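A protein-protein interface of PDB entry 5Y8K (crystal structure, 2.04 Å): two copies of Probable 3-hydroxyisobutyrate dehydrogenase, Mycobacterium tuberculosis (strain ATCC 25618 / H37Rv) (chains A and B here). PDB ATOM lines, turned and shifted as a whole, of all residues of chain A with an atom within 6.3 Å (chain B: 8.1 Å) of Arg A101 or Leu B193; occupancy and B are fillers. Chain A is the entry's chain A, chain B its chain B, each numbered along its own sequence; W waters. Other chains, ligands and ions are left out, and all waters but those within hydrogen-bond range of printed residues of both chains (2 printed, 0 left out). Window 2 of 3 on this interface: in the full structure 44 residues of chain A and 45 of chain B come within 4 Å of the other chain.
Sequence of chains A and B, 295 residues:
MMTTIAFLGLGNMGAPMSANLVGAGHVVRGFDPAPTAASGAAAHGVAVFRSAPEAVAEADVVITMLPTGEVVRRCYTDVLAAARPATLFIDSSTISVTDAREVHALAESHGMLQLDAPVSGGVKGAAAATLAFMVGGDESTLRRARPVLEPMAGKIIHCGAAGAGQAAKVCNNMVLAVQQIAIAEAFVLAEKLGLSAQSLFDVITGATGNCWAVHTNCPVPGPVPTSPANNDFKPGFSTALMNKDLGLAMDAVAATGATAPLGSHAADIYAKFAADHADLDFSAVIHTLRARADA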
ATOM      1  N   SER A  96      14.484  17.538  16.464  1.00  0.00           N
ATOM      2  CA  SER A  96      15.179  17.770  15.207  1.00  0.00           C
ATOM      3  C   SER A  96      15.199  16.512  14.364  1.00  0.00           C
ATOM      4  O   SER A  96      15.153  15.394  14.887  1.00  0.00           O
ATOM      5  CB  SER A  96      16.633  18.272  15.419  1.00  0.00           C
ATOM      6  OG  SER A  96      17.551  17.226  15.771  1.00  0.00           O
ATOM      7  N   VAL A  97      15.252  16.669  13.107  1.00  0.00           N
ATOM      8  CA  VAL A  97      15.378  15.556  12.179  1.00  0.00           C
ATOM      9  C   VAL A  97      16.668  14.771  12.461  1.00  0.00           C
ATOM     10  O   VAL A  97      16.666  13.533  12.423  1.00  0.00           O
ATOM     11  CB  VAL A  97      15.381  16.032  10.715  1.00  0.00           C
ATOM     12  CG1 VAL A  97      15.636  14.864   9.775  1.00  0.00           C
ATOM     13  CG2 VAL A  97      14.068  16.720  10.376  1.00  0.00           C
ATOM     14  N   THR A  98      17.748  15.466  12.790  1.00  0.00           N
ATOM     15  CA  THR A  98      19.028  14.823  13.116  1.00  0.00           C
ATOM     16  C   THR A  98      18.876  13.896  14.317  1.00  0.00           C
ATOM     17  O   THR A  98      19.263  12.712  14.260  1.00  0.00           O
ATOM     18  CB  THR A  98      20.119  15.879  13.404  1.00  0.00           C
ATOM     19  OG1 THR A  98      20.342  16.660  12.218  1.00  0.00           O
ATOM     20  CG2 THR A  98      21.442  15.225  13.832  1.00  0.00           C
ATOM     21  N   ASP A  99      18.302  14.435  15.393  1.00  0.00           N
ATOM     22  CA  ASP A  99      18.065  13.640  16.609  1.00  0.00           C
ATOM     23  C   ASP A  99      17.131  12.469  16.328  1.00  0.00           C
ATOM     24  O   ASP A  99      17.403  11.375  16.764  1.00  0.00           O
ATOM     25  CB  ASP A  99      17.511  14.494  17.754  1.00  0.00           C
ATOM     26  CG  ASP A  99      18.545  15.472  18.325  1.00  0.00           C
ATOM     27  OD1 ASP A  99      19.764  15.336  18.066  1.00  0.00           O
ATOM     28  OD2 ASP A  99      18.133  16.390  19.056  1.00  0.00           O
ATOM     29  N   ALA A 100      16.071  12.692  15.555  1.00  0.00           N
ATOM     30  CA  ALA A 100      15.138  11.627  15.217  1.00  0.00           C
ATOM     31  C   ALA A 100      15.813  10.447  14.538  1.00  0.00           C
ATOM     32  O   ALA A 100      15.576   9.298  14.902  1.00  0.00           O
ATOM     33  CB  ALA A 100      14.027  12.160  14.332  1.00  0.00           C
ATOM     34  N   ARG A 101      16.650  10.749  13.549  1.00  0.00           N
ATOM     35  CA  ARG A 101      17.395   9.722  12.830  1.00  0.00           C
ATOM     36  C   ARG A 101      18.445   9.047  13.701  1.00  0.00           C
ATOM     37  O   ARG A 101      18.694   7.854  13.546  1.00  0.00           O
ATOM     38  CB  ARG A 101      18.026  10.296  11.558  1.00  0.00           C
ATOM     39  CG  ARG A 101      16.995  10.504  10.462  1.00  0.00           C
ATOM     40  CD  ARG A 101      17.520  11.345   9.316  1.00  0.00           C
ATOM     41  NE  ARG A 101      16.491  11.498   8.300  1.00  0.00           N
ATOM     42  CZ  ARG A 101      16.489  12.403   7.323  1.00  0.00           C
ATOM     43  NH1 ARG A 101      17.471  13.304   7.194  1.00  0.00           N
ATOM     44  NH2 ARG A 101      15.470  12.406   6.465  1.00  0.00           N
ATOM     45  N   GLU A 102      19.045   9.780  14.629  1.00  0.00           N
ATOM     46  CA  GLU A 102      19.965   9.142  15.560  1.00  0.00           C
ATOM     47  C   GLU A 102      19.223   8.142  16.444  1.00  0.00           C
ATOM     48  O   GLU A 102      19.676   7.015  16.587  1.00  0.00           O
ATOM     49  CB  GLU A 102      20.712  10.153  16.424  1.00  0.00           C
ATOM     50  CG  GLU A 102      21.864   9.520  17.210  1.00  0.00           C
ATOM     51  CD  GLU A 102      22.518  10.482  18.195  1.00  0.00           C
ATOM     52  OE1 GLU A 102      22.969  10.034  19.275  1.00  0.00           O
ATOM     53  OE2 GLU A 102      22.593  11.687  17.882  1.00  0.00           O
ATOM     54  N   VAL A 103      18.098   8.537  17.040  1.00  0.00           N
ATOM     55  CA  VAL A 103      17.388   7.607  17.942  1.00  0.00           C
ATOM     56  C   VAL A 103      16.789   6.409  17.202  1.00  0.00           C
ATOM     57  O   VAL A 103      16.757   5.317  17.752  1.00  0.00           O
ATOM     58  CB  VAL A 103      16.328   8.280  18.853  1.00  0.00           C
ATOM     59  CG1 VAL A 103      16.990   9.317  19.752  1.00  0.00           C
ATOM     60  CG2 VAL A 103      15.184   8.887  18.061  1.00  0.00           C
ATOM     61  N   HIS A 104      16.369   6.605  15.958  1.00  0.00           N
ATOM     62  CA  HIS A 104      15.861   5.547  15.110  1.00  0.00           C
ATOM     63  C   HIS A 104      16.965   4.502  14.915  1.00  0.00           C
ATOM     64  O   HIS A 104      16.758   3.374  15.181  1.00  0.00           O
ATOM     65  CB  HIS A 104      15.387   6.078  13.759  1.00  0.00           C
ATOM     66  CG  HIS A 104      15.068   5.020  12.762  1.00  0.00           C
ATOM     67  ND1 HIS A 104      13.869   4.361  12.729  1.00  0.00           N
ATOM     68  CD2 HIS A 104      15.795   4.513  11.751  1.00  0.00           C
ATOM     69  CE1 HIS A 104      13.884   3.484  11.756  1.00  0.00           C
ATOM     70  NE2 HIS A 104      15.033   3.570  11.140  1.00  0.00           N
ATOM     71  N   ALA A 105      18.128   4.944  14.453  1.00  0.00           N
ATOM     72  CA  ALA A 105      19.279   4.051  14.247  1.00  0.00           C
ATOM     73  C   ALA A 105      19.644   3.291  15.524  1.00  0.00           C
ATOM     74  O   ALA A 105      19.910   2.085  15.490  1.00  0.00           O
ATOM     75  CB  ALA A 105      20.489   4.839  13.750  1.00  0.00           C
ATOM     76  N   LEU A 106      19.617   3.996  16.647  1.00  0.00           N
ATOM     77  CA  LEU A 106      19.956   3.396  17.935  1.00  0.00           C
ATOM     78  C   LEU A 106      18.998   2.269  18.288  1.00  0.00           C
ATOM     79  O   LEU A 106      19.417   1.174  18.664  1.00  0.00           O
ATOM     80  CB  LEU A 106      19.940   4.474  19.001  1.00  0.00           C
ATOM     81  CG  LEU A 106      20.463   4.150  20.386  1.00  0.00           C
ATOM     82  CD1 LEU A 106      21.924   3.719  20.353  1.00  0.00           C
ATOM     83  CD2 LEU A 106      20.274   5.401  21.225  1.00  0.00           C
ATOM     84  N   ALA A 161      10.983   7.843   4.897  1.00  0.00           N
ATOM     85  CA  ALA A 161      11.885   7.112   5.807  1.00  0.00           C
ATOM     86  C   ALA A 161      12.070   7.864   7.124  1.00  0.00           C
ATOM     87  O   ALA A 161      11.623   9.002   7.271  1.00  0.00           O
ATOM     88  CB  ALA A 161      13.231   6.850   5.137  1.00  0.00           C
ATOM     89  N   ALA A 162      12.712   7.212   8.085  1.00  0.00           N
ATOM     90  CA  ALA A 162      12.909   7.776   9.423  1.00  0.00           C
ATOM     91  C   ALA A 162      13.394   9.224   9.347  1.00  0.00           C
ATOM     92  O   ALA A 162      14.277   9.542   8.551  1.00  0.00           O
ATOM     93  CB  ALA A 162      13.894   6.929  10.223  1.00  0.00           C
ATOM     94  N   GLY A 163      12.788  10.074  10.175  1.00  0.00           N
ATOM     95  CA  GLY A 163      13.011  11.518  10.179  1.00  0.00           C
ATOM     96  C   GLY A 163      12.068  12.374   9.317  1.00  0.00           C
ATOM     97  O   GLY A 163      11.979  13.592   9.514  1.00  0.00           O
ATOM     98  N   ALA A 164      11.381  11.755   8.362  1.00  0.00           N
ATOM     99  CA  ALA A 164      10.503  12.464   7.454  1.00  0.00           C
ATOM    100  C   ALA A 164       9.250  13.003   8.150  1.00  0.00           C
ATOM    101  O   ALA A 164       8.658  13.967   7.670  1.00  0.00           O
ATOM    102  CB  ALA A 164      10.106  11.555   6.287  1.00  0.00           C
ATOM    103  N   ALA A 167      10.487  16.164   9.641  1.00  0.00           N
ATOM    104  CA  ALA A 167      10.800  17.108   8.576  1.00  0.00           C
ATOM    105  C   ALA A 167       9.538  17.721   8.014  1.00  0.00           C
ATOM    106  O   ALA A 167       9.477  18.939   7.785  1.00  0.00           O
ATOM    107  CB  ALA A 167      11.568  16.415   7.464  1.00  0.00           C
ATOM    108  N   VAL A 170       8.036  20.194  10.612  1.00  0.00           N
ATOM    109  CA  VAL A 170       8.809  21.425  10.780  1.00  0.00           C
ATOM    110  C   VAL A 170       8.663  22.321   9.532  1.00  0.00           C
ATOM    111  O   VAL A 170       8.528  23.556   9.662  1.00  0.00           O
ATOM    112  CB  VAL A 170      10.277  21.148  11.241  1.00  0.00           C
ATOM    113  CG1 VAL A 170      11.211  20.745  10.106  1.00  0.00           C
ATOM    114  CG2 VAL A 170      10.822  22.342  12.001  1.00  0.00           C
ATOM    115  N   CYS A 171       8.626  21.706   8.344  1.00  0.00           N
ATOM    116  CA  CYS A 171       8.472  22.484   7.105  1.00  0.00           C
ATOM    117  C   CYS A 171       7.101  23.172   7.024  1.00  0.00           C
ATOM    118  O   CYS A 171       7.024  24.365   6.712  1.00  0.00           O
ATOM    119  CB  CYS A 171       8.749  21.641   5.857  1.00  0.00           C
ATOM    120  SG  CYS A 171      10.491  21.173   5.698  1.00  0.00           S
ATOM    121  N   ALA A 252      17.352  22.763  11.600  1.00  0.00           N
ATOM    122  CA  ALA A 252      17.366  22.084  10.311  1.00  0.00           C
ATOM    123  C   ALA A 252      18.006  22.936   9.187  1.00  0.00           C
ATOM    124  O   ALA A 252      18.770  22.408   8.361  1.00  0.00           O
ATOM    125  CB  ALA A 252      15.968  21.665   9.931  1.00  0.00           C
ATOM    126  N   VAL A 253      17.702  24.238   9.166  1.00  0.00           N
ATOM    127  CA  VAL A 253      18.306  25.167   8.193  1.00  0.00           C
ATOM    128  C   VAL A 253      19.829  25.202   8.377  1.00  0.00           C
ATOM    129  O   VAL A 253      20.563  25.095   7.400  1.00  0.00           O
ATOM    130  CB  VAL A 253      17.699  26.585   8.297  1.00  0.00           C
ATOM    131  CG1 VAL A 253      18.509  27.606   7.494  1.00  0.00           C
ATOM    132  CG2 VAL A 253      16.243  26.581   7.830  1.00  0.00           C
ATOM    133  N   ALA A 255      21.802  22.801   9.997  1.00  0.00           N
ATOM    134  CA  ALA A 255      22.332  21.484   9.684  1.00  0.00           C
ATOM    135  C   ALA A 255      22.473  21.253   8.173  1.00  0.00           C
ATOM    136  O   ALA A 255      23.440  20.639   7.735  1.00  0.00           O
ATOM    137  CB  ALA A 255      21.457  20.406  10.308  1.00  0.00           C
ATOM    138  N   THR A 256      21.515  21.738   7.381  1.00  0.00           N
ATOM    139  CA  THR A 256      21.519  21.496   5.930  1.00  0.00           C
ATOM    140  C   THR A 256      22.260  22.543   5.104  1.00  0.00           C
ATOM    141  O   THR A 256      22.550  22.297   3.944  1.00  0.00           O
ATOM    142  CB  THR A 256      20.089  21.422   5.382  1.00  0.00           C
ATOM    143  OG1 THR A 256      19.394  22.630   5.713  1.00  0.00           O
ATOM    144  CG2 THR A 256      19.350  20.205   5.964  1.00  0.00           C
ATOM    145  N   ALA B 186      10.405  25.983   1.995  1.00  0.00           N
ATOM    146  CA  ALA B 186       9.952  24.708   2.506  1.00  0.00           C
ATOM    147  C   ALA B 186      10.349  23.540   1.593  1.00  0.00           C
ATOM    148  O   ALA B 186      10.884  22.546   2.080  1.00  0.00           O
ATOM    149  CB  ALA B 186       8.440  24.743   2.706  1.00  0.00           C
ATOM    150  N   PHE B 187      10.110  23.663   0.282  1.00  0.00           N
ATOM    151  CA  PHE B 187      10.463  22.577  -0.663  1.00  0.00           C
ATOM    152  C   PHE B 187      11.966  22.311  -0.781  1.00  0.00           C
ATOM    153  O   PHE B 187      12.387  21.147  -0.819  1.00  0.00           O
ATOM    154  CB  PHE B 187       9.839  22.798  -2.056  1.00  0.00           C
ATOM    155  CG  PHE B 187       8.445  22.266  -2.176  1.00  0.00           C
ATOM    156  CD1 PHE B 187       8.227  20.915  -2.407  1.00  0.00           C
ATOM    157  CD2 PHE B 187       7.349  23.102  -2.037  1.00  0.00           C
ATOM    158  CE1 PHE B 187       6.942  20.414  -2.520  1.00  0.00           C
ATOM    159  CE2 PHE B 187       6.053  22.609  -2.138  1.00  0.00           C
ATOM    160  CZ  PHE B 187       5.852  21.260  -2.383  1.00  0.00           C
ATOM    161  N   VAL B 188      12.772  23.373  -0.805  1.00  0.00           N
ATOM    162  CA  VAL B 188      14.220  23.207  -0.869  1.00  0.00           C
ATOM    163  C   VAL B 188      14.758  22.615   0.445  1.00  0.00           C
ATOM    164  O   VAL B 188      15.615  21.741   0.400  1.00  0.00           O
ATOM    165  CB  VAL B 188      14.952  24.506  -1.223  1.00  0.00           C
ATOM    166  CG1 VAL B 188      16.449  24.243  -1.362  1.00  0.00           C
ATOM    167  CG2 VAL B 188      14.462  25.032  -2.558  1.00  0.00           C
ATOM    168  N   LEU B 189      14.256  23.081   1.590  1.00  0.00           N
ATOM    169  CA  LEU B 189      14.668  22.535   2.893  1.00  0.00           C
ATOM    170  C   LEU B 189      14.292  21.065   2.995  1.00  0.00           C
ATOM    171  O   LEU B 189      15.084  20.258   3.482  1.00  0.00           O
ATOM    172  CB  LEU B 189      14.070  23.334   4.057  1.00  0.00           C
ATOM    173  CG  LEU B 189      14.354  22.847   5.481  1.00  0.00           C
ATOM    174  CD1 LEU B 189      15.842  22.864   5.820  1.00  0.00           C
ATOM    175  CD2 LEU B 189      13.563  23.676   6.486  1.00  0.00           C
ATOM    176  N   ALA B 190      13.091  20.722   2.530  1.00  0.00           N
ATOM    177  CA  ALA B 190      12.659  19.333   2.469  1.00  0.00           C
ATOM    178  C   ALA B 190      13.626  18.486   1.652  1.00  0.00           C
ATOM    179  O   ALA B 190      14.031  17.397   2.091  1.00  0.00           O
ATOM    180  CB  ALA B 190      11.254  19.232   1.894  1.00  0.00           C
ATOM    181  N   GLU B 191      14.004  19.000   0.480  1.00  0.00           N
ATOM    182  CA  GLU B 191      14.960  18.324  -0.390  1.00  0.00           C
ATOM    183  C   GLU B 191      16.288  18.075   0.324  1.00  0.00           C
ATOM    184  O   GLU B 191      16.810  16.969   0.254  1.00  0.00           O
ATOM    185  CB  GLU B 191      15.188  19.099  -1.692  1.00  0.00           C
ATOM    186  CG  GLU B 191      16.281  18.502  -2.577  1.00  0.00           C
ATOM    187  N   LYS B 192      16.808  19.076   1.028  1.00  0.00           N
ATOM    188  CA  LYS B 192      18.068  18.905   1.764  1.00  0.00           C
ATOM    189  C   LYS B 192      17.936  17.987   2.991  1.00  0.00           C
ATOM    190  O   LYS B 192      18.926  17.428   3.431  1.00  0.00           O
ATOM    191  CB  LYS B 192      18.659  20.246   2.202  1.00  0.00           C
ATOM    192  CG  LYS B 192      18.948  21.225   1.063  1.00  0.00           C
ATOM    193  CD  LYS B 192      20.046  22.203   1.454  1.00  0.00           C
ATOM    194  CE  LYS B 192      19.967  23.516   0.696  1.00  0.00           C
ATOM    195  NZ  LYS B 192      20.092  23.383  -0.774  1.00  0.00           N
ATOM    196  N   LEU B 193      16.732  17.869   3.551  1.00  0.00           N
ATOM    197  CA  LEU B 193      16.453  16.941   4.663  1.00  0.00           C
ATOM    198  C   LEU B 193      16.150  15.500   4.219  1.00  0.00           C
ATOM    199  O   LEU B 193      15.987  14.624   5.066  1.00  0.00           O
ATOM    200  CB  LEU B 193      15.298  17.465   5.533  1.00  0.00           C
ATOM    201  CG  LEU B 193      15.652  18.691   6.377  1.00  0.00           C
ATOM    202  CD1 LEU B 193      14.391  19.323   6.961  1.00  0.00           C
ATOM    203  CD2 LEU B 193      16.660  18.362   7.479  1.00  0.00           C
ATOM    204  N   GLY B 194      16.083  15.253   2.912  1.00  0.00           N
ATOM    205  CA  GLY B 194      15.664  13.960   2.379  1.00  0.00           C
ATOM    206  C   GLY B 194      14.166  13.676   2.405  1.00  0.00           C
ATOM    207  O   GLY B 194      13.754  12.524   2.270  1.00  0.00           O
ATOM    208  N   LEU B 195      13.353  14.715   2.567  1.00  0.00           N
ATOM    209  CA  LEU B 195      11.906  14.595   2.504  1.00  0.00           C
ATOM    210  C   LEU B 195      11.519  14.823   1.045  1.00  0.00           C
ATOM    211  O   LEU B 195      11.874  15.856   0.491  1.00  0.00           O
ATOM    212  CB  LEU B 195      11.257  15.630   3.437  1.00  0.00           C
ATOM    213  CG  LEU B 195       9.738  15.747   3.425  1.00  0.00           C
ATOM    214  CD1 LEU B 195       9.105  14.453   3.901  1.00  0.00           C
ATOM    215  CD2 LEU B 195       9.274  16.914   4.274  1.00  0.00           C
ATOM    216  N   SER B 196      10.820  13.870   0.414  1.00  0.00           N
ATOM    217  CA  SER B 196      10.440  14.023  -0.997  1.00  0.00           C
ATOM    218  C   SER B 196       9.451  15.181  -1.223  1.00  0.00           C
ATOM    219  O   SER B 196       8.636  15.512  -0.348  1.00  0.00           O
ATOM    220  CB  SER B 196       9.845  12.730  -1.575  1.00  0.00           C
ATOM    221  OG  SER B 196       8.482  12.577  -1.212  1.00  0.00           O
HETATM  222  O   HOH W   1      19.263  15.180   5.308  1.00  0.00           O
HETATM  223  O   HOH W   2      12.150  10.076   3.070  1.00  0.00           O
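Of the 22 printed residues of chain A, 6 touch a printed residue of chain B.
Hydrophobic or aromatic side chains of chain A that line the printed part of chain B: Ala A164 and Ala A167.
Among the printed residues, 8 pairs touch across the chains.
Among the printed residues, no Asp or Glu carboxylate lies within 4 Å of a Lys or Arg side-chain nitrogen of the other chain.
No position is printed for both chains.
Ala A164 touches Leu B195.
CD2 of Leu B195 touches C of Ala A167, at 3.8 Å.
Cys A171 touches Ala B186 (SG to O, 3.9 Å).
CD1 of Leu B189 touches O of Ala A252, 3.9 Å away.
OG1 of Thr A256 touches CD1 of Leu B189 (3.6 Å).
Lys B192 touches Thr A256 (CD to O, 3.5 Å).
CG2 of Thr A256 touches CD2 of Leu B193, at 3.6 Å.
Water W1 lies within hydrogen-bond range of the backbone carbonyl oxygen of Lys B192 (2.9 Å), the guanidinium group of Arg A101 (3.2 Å) and the backbone carbonyl oxygen of Leu B193 (3.3 Å).
Water W2 bridges the backbone carbonyl oxygen of Gly B194 and the backbone NH of Ala A161.
The backbone carbonyl oxygen (O) of Leu B193 sits at hydrogen-bond distance from the guanidinium group (NH2) of Arg A101 (2.7 Å).
Arg A101 touches just one residue of chain B: Leu B193.
Of the printed residues of chain A, Leu B193 touches Arg A101 (2.7 Å) and Thr A256 (3.6 Å).
No residue of chain B comes within 4 Å of Ala A100.
Of the printed residues of chain A, Leu B195 touches Ala A164 (3.8 Å) and Ala A167 (3.8 Å).
Of the printed residues of chain B, Ala A167 touches Leu B195.
Ser A96 touches none of the printed residues of chain B.
Glu B191 touches none of the printed residues of chain A.
The guanidinium group of Arg A101 is in hydrogen-bond range of the backbone carbonyl oxygen of Ala A162.
The backbone carbonyl oxygen (O) of Ala A167 is in hydrogen-bond range of the side-chain sulfur (SG) of Cys A171.
O of Ala A252 is in hydrogen-bond range of OG1 of Thr A256 (2.7 Å).
The side-chain hydroxyl (OG1) of Thr A256 lies within hydrogen-bond range of the backbone carbonyl oxygen (O) of Val A253 (3.2 Å).
The backbone NH (N) of Leu B195 sits at hydrogen-bond distance from the backbone carbonyl oxygen (O) of Ala B190 (2.8 Å).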
